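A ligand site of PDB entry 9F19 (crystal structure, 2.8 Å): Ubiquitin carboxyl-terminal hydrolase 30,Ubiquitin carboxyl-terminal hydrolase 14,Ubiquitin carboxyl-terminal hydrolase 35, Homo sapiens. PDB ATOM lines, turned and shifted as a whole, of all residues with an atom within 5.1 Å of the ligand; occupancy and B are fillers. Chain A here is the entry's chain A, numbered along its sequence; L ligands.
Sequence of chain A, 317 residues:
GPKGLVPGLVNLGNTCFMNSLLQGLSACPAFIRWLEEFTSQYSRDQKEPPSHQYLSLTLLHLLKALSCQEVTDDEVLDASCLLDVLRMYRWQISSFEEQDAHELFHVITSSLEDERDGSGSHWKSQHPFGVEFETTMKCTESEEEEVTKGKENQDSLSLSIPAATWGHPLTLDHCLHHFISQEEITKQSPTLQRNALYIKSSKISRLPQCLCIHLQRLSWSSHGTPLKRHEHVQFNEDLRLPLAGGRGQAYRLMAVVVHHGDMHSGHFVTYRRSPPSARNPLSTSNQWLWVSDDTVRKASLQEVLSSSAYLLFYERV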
ATOM      1  N   ASN A  14      13.682  30.074  34.520  1.00  0.00           N
ATOM      2  CA  ASN A  14      13.320  28.694  34.233  1.00  0.00           C
ATOM      3  C   ASN A  14      14.363  27.803  34.903  1.00  0.00           C
ATOM      4  O   ASN A  14      15.516  27.772  34.476  1.00  0.00           O
ATOM      5  CB  ASN A  14      13.271  28.434  32.726  1.00  0.00           C
ATOM      6  CG  ASN A  14      12.501  27.183  32.379  1.00  0.00           C
ATOM      7  OD1 ASN A  14      12.225  26.335  33.243  1.00  0.00           O
ATOM      8  ND2 ASN A  14      12.171  27.036  31.097  1.00  0.00           N
ATOM      9  N   THR A  15      13.967  27.142  35.993  1.00  0.00           N
ATOM     10  CA  THR A  15      14.837  26.147  36.618  1.00  0.00           C
ATOM     11  C   THR A  15      14.055  24.915  37.011  1.00  0.00           C
ATOM     12  O   THR A  15      14.688  23.892  37.301  1.00  0.00           O
ATOM     13  CB  THR A  15      15.564  26.710  37.850  1.00  0.00           C
ATOM     14  OG1 THR A  15      15.883  28.086  37.648  1.00  0.00           O
ATOM     15  CG2 THR A  15      16.896  25.984  38.089  1.00  0.00           C
ATOM     16  N   CYS A  16      12.716  24.942  36.911  1.00  0.00           N
ATOM     17  CA  CYS A  16      11.801  24.059  37.642  1.00  0.00           C
ATOM     18  C   CYS A  16      12.129  22.591  37.496  1.00  0.00           C
ATOM     19  O   CYS A  16      12.068  21.843  38.469  1.00  0.00           O
ATOM     20  CB  CYS A  16      10.377  24.281  37.154  1.00  0.00           C
ATOM     21  SG  CYS A  16       9.263  25.289  38.128  1.00  0.00           S
ATOM     22  N   PHE A  17      12.495  22.169  36.270  1.00  0.00           N
ATOM     23  CA  PHE A  17      12.862  20.771  36.072  1.00  0.00           C
ATOM     24  C   PHE A  17      14.122  20.408  36.841  1.00  0.00           C
ATOM     25  O   PHE A  17      14.205  19.316  37.389  1.00  0.00           O
ATOM     26  CB  PHE A  17      13.102  20.420  34.604  1.00  0.00           C
ATOM     27  CG  PHE A  17      13.614  19.007  34.436  1.00  0.00           C
ATOM     28  CD1 PHE A  17      12.781  17.941  34.689  1.00  0.00           C
ATOM     29  CD2 PHE A  17      14.932  18.751  34.132  1.00  0.00           C
ATOM     30  CE1 PHE A  17      13.249  16.630  34.566  1.00  0.00           C
ATOM     31  CE2 PHE A  17      15.398  17.472  34.036  1.00  0.00           C
ATOM     32  CZ  PHE A  17      14.569  16.403  34.246  1.00  0.00           C
ATOM     33  N   MET A  18      15.130  21.294  36.847  1.00  0.00           N
ATOM     34  CA  MET A  18      16.376  20.974  37.540  1.00  0.00           C
ATOM     35  C   MET A  18      16.137  20.785  39.035  1.00  0.00           C
ATOM     36  O   MET A  18      16.611  19.804  39.617  1.00  0.00           O
ATOM     37  CB  MET A  18      17.439  22.035  37.327  1.00  0.00           C
ATOM     38  CG  MET A  18      18.711  21.732  38.125  1.00  0.00           C
ATOM     39  SD  MET A  18      20.094  22.781  37.670  1.00  0.00           S
ATOM     40  CE  MET A  18      20.365  22.177  35.998  1.00  0.00           C
ATOM     41  N   LEU A  83      24.358  24.942  37.902  1.00  0.00           N
ATOM     42  CA  LEU A  83      24.390  25.561  36.583  1.00  0.00           C
ATOM     43  C   LEU A  83      25.761  26.160  36.290  1.00  0.00           C
ATOM     44  O   LEU A  83      26.244  26.096  35.153  1.00  0.00           O
ATOM     45  CB  LEU A  83      23.328  26.648  36.458  1.00  0.00           C
ATOM     46  CG  LEU A  83      21.876  26.264  36.245  1.00  0.00           C
ATOM     47  CD1 LEU A  83      21.184  26.150  37.576  1.00  0.00           C
ATOM     48  CD2 LEU A  83      21.262  27.389  35.454  1.00  0.00           C
ATOM     49  N   ILE A  93      23.783  25.564  28.758  1.00  0.00           N
ATOM     50  CA  ILE A  93      22.532  25.107  29.353  1.00  0.00           C
ATOM     51  C   ILE A  93      21.308  25.781  28.742  1.00  0.00           C
ATOM     52  O   ILE A  93      20.236  25.172  28.726  1.00  0.00           O
ATOM     53  CB  ILE A  93      22.562  25.258  30.883  1.00  0.00           C
ATOM     54  CG1 ILE A  93      23.295  26.523  31.382  1.00  0.00           C
ATOM     55  CG2 ILE A  93      23.168  23.995  31.491  1.00  0.00           C
ATOM     56  CD1 ILE A  93      22.573  27.888  31.150  1.00  0.00           C
ATOM     57  N   SER A  94      21.462  26.987  28.181  1.00  0.00           N
ATOM     58  CA  SER A  94      20.317  27.686  27.630  1.00  0.00           C
ATOM     59  C   SER A  94      19.765  27.026  26.383  1.00  0.00           C
ATOM     60  O   SER A  94      18.698  27.423  25.937  1.00  0.00           O
ATOM     61  CB  SER A  94      20.669  29.140  27.313  1.00  0.00           C
ATOM     62  N   PHE A  96      19.131  23.787  26.440  1.00  0.00           N
ATOM     63  CA  PHE A  96      18.426  22.606  26.942  1.00  0.00           C
ATOM     64  C   PHE A  96      16.960  22.839  27.244  1.00  0.00           C
ATOM     65  O   PHE A  96      16.212  21.868  27.366  1.00  0.00           O
ATOM     66  CB  PHE A  96      19.110  22.079  28.199  1.00  0.00           C
ATOM     67  CG  PHE A  96      20.283  21.223  27.905  1.00  0.00           C
ATOM     68  CD1 PHE A  96      20.105  20.001  27.266  1.00  0.00           C
ATOM     69  CD2 PHE A  96      21.559  21.628  28.229  1.00  0.00           C
ATOM     70  CE1 PHE A  96      21.175  19.190  26.968  1.00  0.00           C
ATOM     71  CE2 PHE A  96      22.638  20.835  27.926  1.00  0.00           C
ATOM     72  CZ  PHE A  96      22.447  19.609  27.291  1.00  0.00           C
ATOM     73  N   GLU A  97      16.525  24.092  27.337  1.00  0.00           N
ATOM     74  CA  GLU A  97      15.101  24.372  27.465  1.00  0.00           C
ATOM     75  C   GLU A  97      14.361  24.137  26.160  1.00  0.00           C
ATOM     76  O   GLU A  97      13.129  24.076  26.164  1.00  0.00           O
ATOM     77  CB  GLU A  97      14.877  25.813  27.934  1.00  0.00           C
ATOM     78  CG  GLU A  97      15.914  26.796  27.438  1.00  0.00           C
ATOM     79  CD  GLU A  97      15.677  28.234  27.911  1.00  0.00           C
ATOM     80  OE1 GLU A  97      14.499  28.656  27.987  1.00  0.00           O
ATOM     81  OE2 GLU A  97      16.672  28.943  28.200  1.00  0.00           O
ATOM     82  N   GLU A  98      15.074  24.029  25.049  1.00  0.00           N
ATOM     83  CA  GLU A  98      14.452  23.705  23.783  1.00  0.00           C
ATOM     84  C   GLU A  98      14.367  22.209  23.543  1.00  0.00           C
ATOM     85  O   GLU A  98      13.741  21.793  22.554  1.00  0.00           O
ATOM     86  CB  GLU A  98      15.208  24.383  22.624  1.00  0.00           C
ATOM     87  CG  GLU A  98      15.837  25.728  22.988  1.00  0.00           C
ATOM     88  CD  GLU A  98      16.969  26.105  22.029  1.00  0.00           C
ATOM     89  OE1 GLU A  98      17.410  25.234  21.235  1.00  0.00           O
ATOM     90  OE2 GLU A  98      17.424  27.272  22.079  1.00  0.00           O
ATOM     91  N   GLN A  99      14.965  21.392  24.390  1.00  0.00           N
ATOM     92  CA  GLN A  99      14.910  19.953  24.237  1.00  0.00           C
ATOM     93  C   GLN A  99      13.993  19.361  25.316  1.00  0.00           C
ATOM     94  O   GLN A  99      13.436  20.082  26.152  1.00  0.00           O
ATOM     95  CB  GLN A  99      16.324  19.353  24.290  1.00  0.00           C
ATOM     96  CG  GLN A  99      17.363  20.124  23.485  1.00  0.00           C
ATOM     97  CD  GLN A  99      17.016  20.271  22.002  1.00  0.00           C
ATOM     98  OE1 GLN A  99      16.420  19.371  21.410  1.00  0.00           O
ATOM     99  NE2 GLN A  99      17.418  21.396  21.405  1.00  0.00           N
ATOM    100  N   ASP A 100      13.821  18.039  25.266  1.00  0.00           N
ATOM    101  CA  ASP A 100      13.128  17.336  26.320  1.00  0.00           C
ATOM    102  C   ASP A 100      13.910  17.456  27.613  1.00  0.00           C
ATOM    103  O   ASP A 100      15.143  17.457  27.598  1.00  0.00           O
ATOM    104  CB  ASP A 100      12.978  15.867  25.945  1.00  0.00           C
ATOM    105  CG  ASP A 100      12.012  15.123  26.842  1.00  0.00           C
ATOM    106  OD1 ASP A 100      11.074  15.766  27.377  1.00  0.00           O
ATOM    107  OD2 ASP A 100      12.199  13.902  27.022  1.00  0.00           O
ATOM    108  N   ALA A 101      13.181  17.575  28.736  1.00  0.00           N
ATOM    109  CA  ALA A 101      13.801  17.768  30.056  1.00  0.00           C
ATOM    110  C   ALA A 101      14.761  16.655  30.408  1.00  0.00           C
ATOM    111  O   ALA A 101      15.831  16.911  30.994  1.00  0.00           O
ATOM    112  CB  ALA A 101      12.731  17.852  31.142  1.00  0.00           C
ATOM    113  N   LEU A 104      18.692  16.612  30.181  1.00  0.00           N
ATOM    114  CA  LEU A 104      19.513  17.142  31.250  1.00  0.00           C
ATOM    115  C   LEU A 104      19.982  16.029  32.167  1.00  0.00           C
ATOM    116  O   LEU A 104      21.149  16.012  32.589  1.00  0.00           O
ATOM    117  CB  LEU A 104      18.745  18.198  32.039  1.00  0.00           C
ATOM    118  CG  LEU A 104      19.543  18.759  33.223  1.00  0.00           C
ATOM    119  CD1 LEU A 104      20.441  19.884  32.758  1.00  0.00           C
ATOM    120  CD2 LEU A 104      18.605  19.237  34.306  1.00  0.00           C
ATOM    121  N   ARG A 217       6.397  11.348  27.297  1.00  0.00           N
ATOM    122  CA  ARG A 217       5.201  12.169  27.260  1.00  0.00           C
ATOM    123  C   ARG A 217       5.213  13.158  26.133  1.00  0.00           C
ATOM    124  O   ARG A 217       4.157  13.729  25.843  1.00  0.00           O
ATOM    125  CB  ARG A 217       5.025  12.943  28.558  1.00  0.00           C
ATOM    126  CG  ARG A 217       4.619  12.048  29.690  1.00  0.00           C
ATOM    127  CD  ARG A 217       3.636  12.684  30.611  1.00  0.00           C
ATOM    128  NE  ARG A 217       3.234  11.721  31.629  1.00  0.00           N
ATOM    129  CZ  ARG A 217       2.092  11.075  31.646  1.00  0.00           C
ATOM    130  NH1 ARG A 217       1.172  11.282  30.728  1.00  0.00           N
ATOM    131  NH2 ARG A 217       1.846  10.226  32.638  1.00  0.00           N
ATOM    132  N   LEU A 218       6.358  13.393  25.507  1.00  0.00           N
ATOM    133  CA  LEU A 218       6.480  14.324  24.395  1.00  0.00           C
ATOM    134  C   LEU A 218       6.524  13.541  23.088  1.00  0.00           C
ATOM    135  O   LEU A 218       7.523  12.884  22.771  1.00  0.00           O
ATOM    136  CB  LEU A 218       7.718  15.203  24.597  1.00  0.00           C
ATOM    137  CG  LEU A 218       7.495  16.695  24.391  1.00  0.00           C
ATOM    138  CD1 LEU A 218       6.251  17.090  25.155  1.00  0.00           C
ATOM    139  CD2 LEU A 218       8.719  17.536  24.843  1.00  0.00           C
ATOM    140  N   TRP A 220       5.672  13.309  18.705  1.00  0.00           N
ATOM    141  CA  TRP A 220       5.761  14.155  17.522  1.00  0.00           C
ATOM    142  C   TRP A 220       4.886  13.601  16.397  1.00  0.00           C
ATOM    143  O   TRP A 220       4.993  12.429  16.046  1.00  0.00           O
ATOM    144  CB  TRP A 220       7.227  14.255  17.070  1.00  0.00           C
ATOM    145  CG  TRP A 220       8.065  15.116  17.966  1.00  0.00           C
ATOM    146  CD1 TRP A 220       8.521  14.809  19.220  1.00  0.00           C
ATOM    147  CD2 TRP A 220       8.520  16.428  17.679  1.00  0.00           C
ATOM    148  NE1 TRP A 220       9.252  15.863  19.734  1.00  0.00           N
ATOM    149  CE2 TRP A 220       9.265  16.861  18.803  1.00  0.00           C
ATOM    150  CE3 TRP A 220       8.379  17.283  16.591  1.00  0.00           C
ATOM    151  CZ2 TRP A 220       9.860  18.123  18.856  1.00  0.00           C
ATOM    152  CZ3 TRP A 220       8.977  18.531  16.635  1.00  0.00           C
ATOM    153  CH2 TRP A 220       9.699  18.939  17.759  1.00  0.00           C
ATOM    154  N   PRO A 226       5.088  18.893  17.548  1.00  0.00           N
ATOM    155  CA  PRO A 226       5.106  18.128  18.797  1.00  0.00           C
ATOM    156  C   PRO A 226       3.849  18.299  19.632  1.00  0.00           C
ATOM    157  O   PRO A 226       3.134  19.302  19.542  1.00  0.00           O
ATOM    158  CB  PRO A 226       6.320  18.704  19.545  1.00  0.00           C
ATOM    159  CG  PRO A 226       6.440  20.069  19.049  1.00  0.00           C
ATOM    160  CD  PRO A 226       5.909  20.119  17.647  1.00  0.00           C
ATOM    161  N   LYS A 228       1.998  16.925  23.691  1.00  0.00           N
ATOM    162  CA  LYS A 228       2.150  16.273  24.993  1.00  0.00           C
ATOM    163  C   LYS A 228       1.032  15.267  25.189  1.00  0.00           C
ATOM    164  O   LYS A 228      -0.153  15.592  25.023  1.00  0.00           O
ATOM    165  CB  LYS A 228       2.129  17.285  26.141  1.00  0.00           C
ATOM    166  CG  LYS A 228       1.664  16.724  27.472  1.00  0.00           C
ATOM    167  CD  LYS A 228       1.869  17.712  28.622  1.00  0.00           C
ATOM    168  CE  LYS A 228       1.605  17.050  29.973  1.00  0.00           C
ATOM    169  NZ  LYS A 228       1.397  18.039  31.087  1.00  0.00           N
ATOM    170  N   ARG A 229       1.408  14.035  25.523  1.00  0.00           N
ATOM    171  CA  ARG A 229       0.461  13.009  25.932  1.00  0.00           C
ATOM    172  C   ARG A 229       0.084  13.227  27.392  1.00  0.00           C
ATOM    173  O   ARG A 229       0.955  13.203  28.271  1.00  0.00           O
ATOM    174  CB  ARG A 229       1.081  11.617  25.735  1.00  0.00           C
ATOM    175  CG  ARG A 229       1.363  11.237  24.272  1.00  0.00           C
ATOM    176  CD  ARG A 229       0.786   9.852  23.933  1.00  0.00           C
ATOM    177  NE  ARG A 229      -0.460   9.611  24.657  1.00  0.00           N
ATOM    178  CZ  ARG A 229      -1.020   8.417  24.824  1.00  0.00           C
ATOM    179  NH1 ARG A 229      -0.467   7.317  24.334  1.00  0.00           N
ATOM    180  NH2 ARG A 229      -2.168   8.319  25.491  1.00  0.00           N
ATOM    181  N   HIS A 259       4.820  16.675  35.151  1.00  0.00           N
ATOM    182  CA  HIS A 259       4.732  17.897  34.364  1.00  0.00           C
ATOM    183  C   HIS A 259       3.294  18.410  34.290  1.00  0.00           C
ATOM    184  O   HIS A 259       2.355  17.619  34.126  1.00  0.00           O
ATOM    185  CB  HIS A 259       5.239  17.704  32.931  1.00  0.00           C
ATOM    186  CG  HIS A 259       5.154  18.962  32.116  1.00  0.00           C
ATOM    187  ND1 HIS A 259       4.092  19.223  31.275  1.00  0.00           N
ATOM    188  CD2 HIS A 259       5.996  20.022  32.019  1.00  0.00           C
ATOM    189  CE1 HIS A 259       4.275  20.401  30.701  1.00  0.00           C
ATOM    190  NE2 HIS A 259       5.424  20.904  31.123  1.00  0.00           N
ATOM    191  N   MET A 263       3.143  21.889  26.755  1.00  0.00           N
ATOM    192  CA  MET A 263       4.508  21.379  26.638  1.00  0.00           C
ATOM    193  C   MET A 263       5.566  22.463  26.828  1.00  0.00           C
ATOM    194  O   MET A 263       6.617  22.209  27.431  1.00  0.00           O
ATOM    195  CB  MET A 263       4.683  20.684  25.295  1.00  0.00           C
ATOM    196  CG  MET A 263       4.091  21.488  24.167  1.00  0.00           C
ATOM    197  SD  MET A 263       3.978  20.576  22.628  1.00  0.00           S
ATOM    198  CE  MET A 263       4.359  21.897  21.472  1.00  0.00           C
ATOM    199  N   HIS A 264       5.282  23.694  26.358  1.00  0.00           N
ATOM    200  CA  HIS A 264       6.225  24.798  26.468  1.00  0.00           C
ATOM    201  C   HIS A 264       6.205  25.453  27.843  1.00  0.00           C
ATOM    202  O   HIS A 264       7.047  26.316  28.101  1.00  0.00           O
ATOM    203  CB  HIS A 264       5.931  25.857  25.403  1.00  0.00           C
ATOM    204  CG  HIS A 264       6.269  25.405  24.023  1.00  0.00           C
ATOM    205  ND1 HIS A 264       7.383  24.627  23.750  1.00  0.00           N
ATOM    206  CD2 HIS A 264       5.636  25.587  22.842  1.00  0.00           C
ATOM    207  CE1 HIS A 264       7.427  24.372  22.459  1.00  0.00           C
ATOM    208  NE2 HIS A 264       6.379  24.937  21.876  1.00  0.00           N
ATOM    209  N   SER A 265       5.250  25.100  28.693  1.00  0.00           N
ATOM    210  CA  SER A 265       5.335  25.486  30.098  1.00  0.00           C
ATOM    211  C   SER A 265       6.388  24.630  30.791  1.00  0.00           C
ATOM    212  O   SER A 265       6.564  23.447  30.477  1.00  0.00           O
ATOM    213  CB  SER A 265       3.991  25.306  30.794  1.00  0.00           C
ATOM    214  OG  SER A 265       3.890  24.016  31.388  1.00  0.00           O
ATOM    215  N   GLY A 266       7.078  25.231  31.734  1.00  0.00           N
ATOM    216  CA  GLY A 266       8.132  24.511  32.424  1.00  0.00           C
ATOM    217  C   GLY A 266       7.699  24.047  33.793  1.00  0.00           C
ATOM    218  O   GLY A 266       8.531  23.941  34.685  1.00  0.00           O
ATOM    219  N   PHE A 268       7.248  21.856  36.486  1.00  0.00           N
ATOM    220  CA  PHE A 268       7.688  20.543  36.923  1.00  0.00           C
ATOM    221  C   PHE A 268       7.652  20.458  38.435  1.00  0.00           C
ATOM    222  O   PHE A 268       8.129  21.361  39.129  1.00  0.00           O
ATOM    223  CB  PHE A 268       9.106  20.254  36.423  1.00  0.00           C
ATOM    224  CG  PHE A 268       9.170  19.835  34.988  1.00  0.00           C
ATOM    225  CD1 PHE A 268       8.804  18.561  34.622  1.00  0.00           C
ATOM    226  CD2 PHE A 268       9.655  20.704  34.018  1.00  0.00           C
ATOM    227  CE1 PHE A 268       8.873  18.162  33.307  1.00  0.00           C
ATOM    228  CE2 PHE A 268       9.744  20.303  32.688  1.00  0.00           C
ATOM    229  CZ  PHE A 268       9.339  19.038  32.330  1.00  0.00           C
ATOM    230  N   TYR A 310       5.945  11.667  34.832  1.00  0.00           N
ATOM    231  CA  TYR A 310       6.944  11.877  33.787  1.00  0.00           C
ATOM    232  C   TYR A 310       8.237  11.126  34.071  1.00  0.00           C
ATOM    233  O   TYR A 310       8.674  10.325  33.236  1.00  0.00           O
ATOM    234  CB  TYR A 310       7.231  13.374  33.635  1.00  0.00           C
ATOM    235  CG  TYR A 310       8.339  13.733  32.653  1.00  0.00           C
ATOM    236  CD1 TYR A 310       8.235  13.406  31.305  1.00  0.00           C
ATOM    237  CD2 TYR A 310       9.456  14.421  33.073  1.00  0.00           C
ATOM    238  CE1 TYR A 310       9.233  13.748  30.405  1.00  0.00           C
ATOM    239  CE2 TYR A 310      10.461  14.773  32.179  1.00  0.00           C
ATOM    240  CZ  TYR A 310      10.339  14.426  30.850  1.00  0.00           C
ATOM    241  OH  TYR A 310      11.368  14.773  29.983  1.00  0.00           O
HETATM  242  C1  LIG L   1      10.272  22.113  26.468  1.00  0.00           C
HETATM  243  C2  LIG L   1      10.006  21.539  25.106  1.00  0.00           C
HETATM  244  C3  LIG L   1       8.694  21.350  24.640  1.00  0.00           C
HETATM  245  C4  LIG L   1       8.480  20.801  23.376  1.00  0.00           C
HETATM  246  C5  LIG L   1       9.558  20.449  22.572  1.00  0.00           C
HETATM  247  C6  LIG L   1      10.867  20.630  23.041  1.00  0.00           C
HETATM  248  C7  LIG L   1      11.090  21.173  24.303  1.00  0.00           C
HETATM  249  C8  LIG L   1       9.365  18.990  28.404  1.00  0.00           C
HETATM  250  C9  LIG L   1       8.106  18.247  28.653  1.00  0.00           C
HETATM  251  C10 LIG L   1       8.217  17.016  29.322  1.00  0.00           C
HETATM  252  C11 LIG L   1       7.061  16.288  29.595  1.00  0.00           C
HETATM  253  C12 LIG L   1       5.821  16.778  29.196  1.00  0.00           C
HETATM  254  C13 LIG L   1       5.701  17.973  28.504  1.00  0.00           C
HETATM  255  C14 LIG L   1       6.845  18.731  28.280  1.00  0.00           C
HETATM  256  C15 LIG L   1      14.850  22.698  32.023  1.00  0.00           C
HETATM  257  C16 LIG L   1      13.647  23.380  31.885  1.00  0.00           C
HETATM  258  C17 LIG L   1      12.799  23.082  30.826  1.00  0.00           C
HETATM  259  C18 LIG L   1      13.159  22.088  29.905  1.00  0.00           C
HETATM  260  C19 LIG L   1      10.993  21.530  28.809  1.00  0.00           C
HETATM  261  C20 LIG L   1      10.503  20.975  27.467  1.00  0.00           C
HETATM  262  C21 LIG L   1      14.372  21.391  30.085  1.00  0.00           C
HETATM  263  C22 LIG L   1      15.226  21.704  31.130  1.00  0.00           C
HETATM  264  C23 LIG L   1      17.312  25.064  31.934  1.00  0.00           C
HETATM  265  C24 LIG L   1      17.527  24.463  30.546  1.00  0.00           C
HETATM  266  C25 LIG L   1      16.125  26.022  31.871  1.00  0.00           C
HETATM  267  C26 LIG L   1      18.534  25.898  32.398  1.00  0.00           C
HETATM  268  F1  LIG L   1       4.706  16.093  29.442  1.00  0.00           F
HETATM  269  N1  LIG L   1      12.370  21.668  28.831  1.00  0.00           N
HETATM  270  N2  LIG L   1       9.301  20.184  27.720  1.00  0.00           N
HETATM  271  N3  LIG L   1      17.247  23.970  32.924  1.00  0.00           N
HETATM  272  O1  LIG L   1      15.069  24.073  34.179  1.00  0.00           O
HETATM  273  O2  LIG L   1      10.434  18.533  28.839  1.00  0.00           O
HETATM  274  O3  LIG L   1      10.186  21.761  29.714  1.00  0.00           O
HETATM  275  O4  LIG L   1      18.516  27.213  31.902  1.00  0.00           O
HETATM  276  O5  LIG L   1      16.209  21.873  34.075  1.00  0.00           O
HETATM  277  S1  LIG L   1      15.875  23.131  33.414  1.00  0.00           S
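N of Met 18 sits at hydrogen-bond distance from O5 of the ligand, at 3.0 Å. N of Ala 101 is in hydrogen-bond range of O2 of the ligand, at 2.9 Å. A nitrogen (N1) of the ligand lies close to the backbone carbonyl oxygen of Gln 99, 3.3 Å away. A nitrogen (N2) of the ligand sits at hydrogen-bond distance from the backbone carbonyl oxygen of Met 263 (3.4 Å).
OD1 of Asp 100 lies within hydrogen-bond range of OH of Tyr 310, at 2.8 Å. The side-chain sulfur (SG) of Cys 16 sits close to the backbone carbonyl oxygen (O) of Gly 266 (3.8 Å). ND1 of His 259 is in hydrogen-bond range of NZ of Lys 228 (2.9 Å). NE2 of His 259 is in hydrogen-bond range of O of Ser 265, at 2.9 Å. The backbone carbonyl oxygen (O) of Arg 217 is in hydrogen-bond range of the backbone NH (N) of Arg 229, 2.8 Å away.
An oxygen (O1) of the ligand sits close to the backbone carbonyl oxygen of Thr 15 (3.2 Å). The side-chain carboxylate of Asp 100 lies close to an oxygen (O2) of the ligand (3.2 Å). Asn 14 touches the ligand. Cys 16 touches the ligand. Phe 17 touches the ligand. O of Ile 93 touches C24 of the ligand, at 3.3 Å. Phe 96 touches the ligand (O to C21, 3.3 Å). Glu 97 touches the ligand. Glu 98 touches the ligand. Leu 104 touches the ligand. Arg 217 touches the ligand (CB to F1, 3.3 Å). Leu 218 touches the ligand (CD1 to C13, 3.5 Å). CE of Lys 228 touches F1 of the ligand (3.3 Å). His 259 touches the ligand (ND1 to C13, 3.4 Å). ND1 of His 264 touches C3 of the ligand, at 3.6 Å. Phe 268 touches the ligand (CE2 to O3, 3.3 Å). Tyr 310 touches the ligand (CE1 to C11, 3.4 Å). Hydrophobic or aromatic side chains within 4 Å of the ligand: Phe 17, Met 18, Phe 96, Ala 101, Leu 104, Leu 218, His 259, His 264, Phe 268 and Tyr 310. The nearest printed residue that does not touch the ligand is Ser 265 (4.1 Å).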
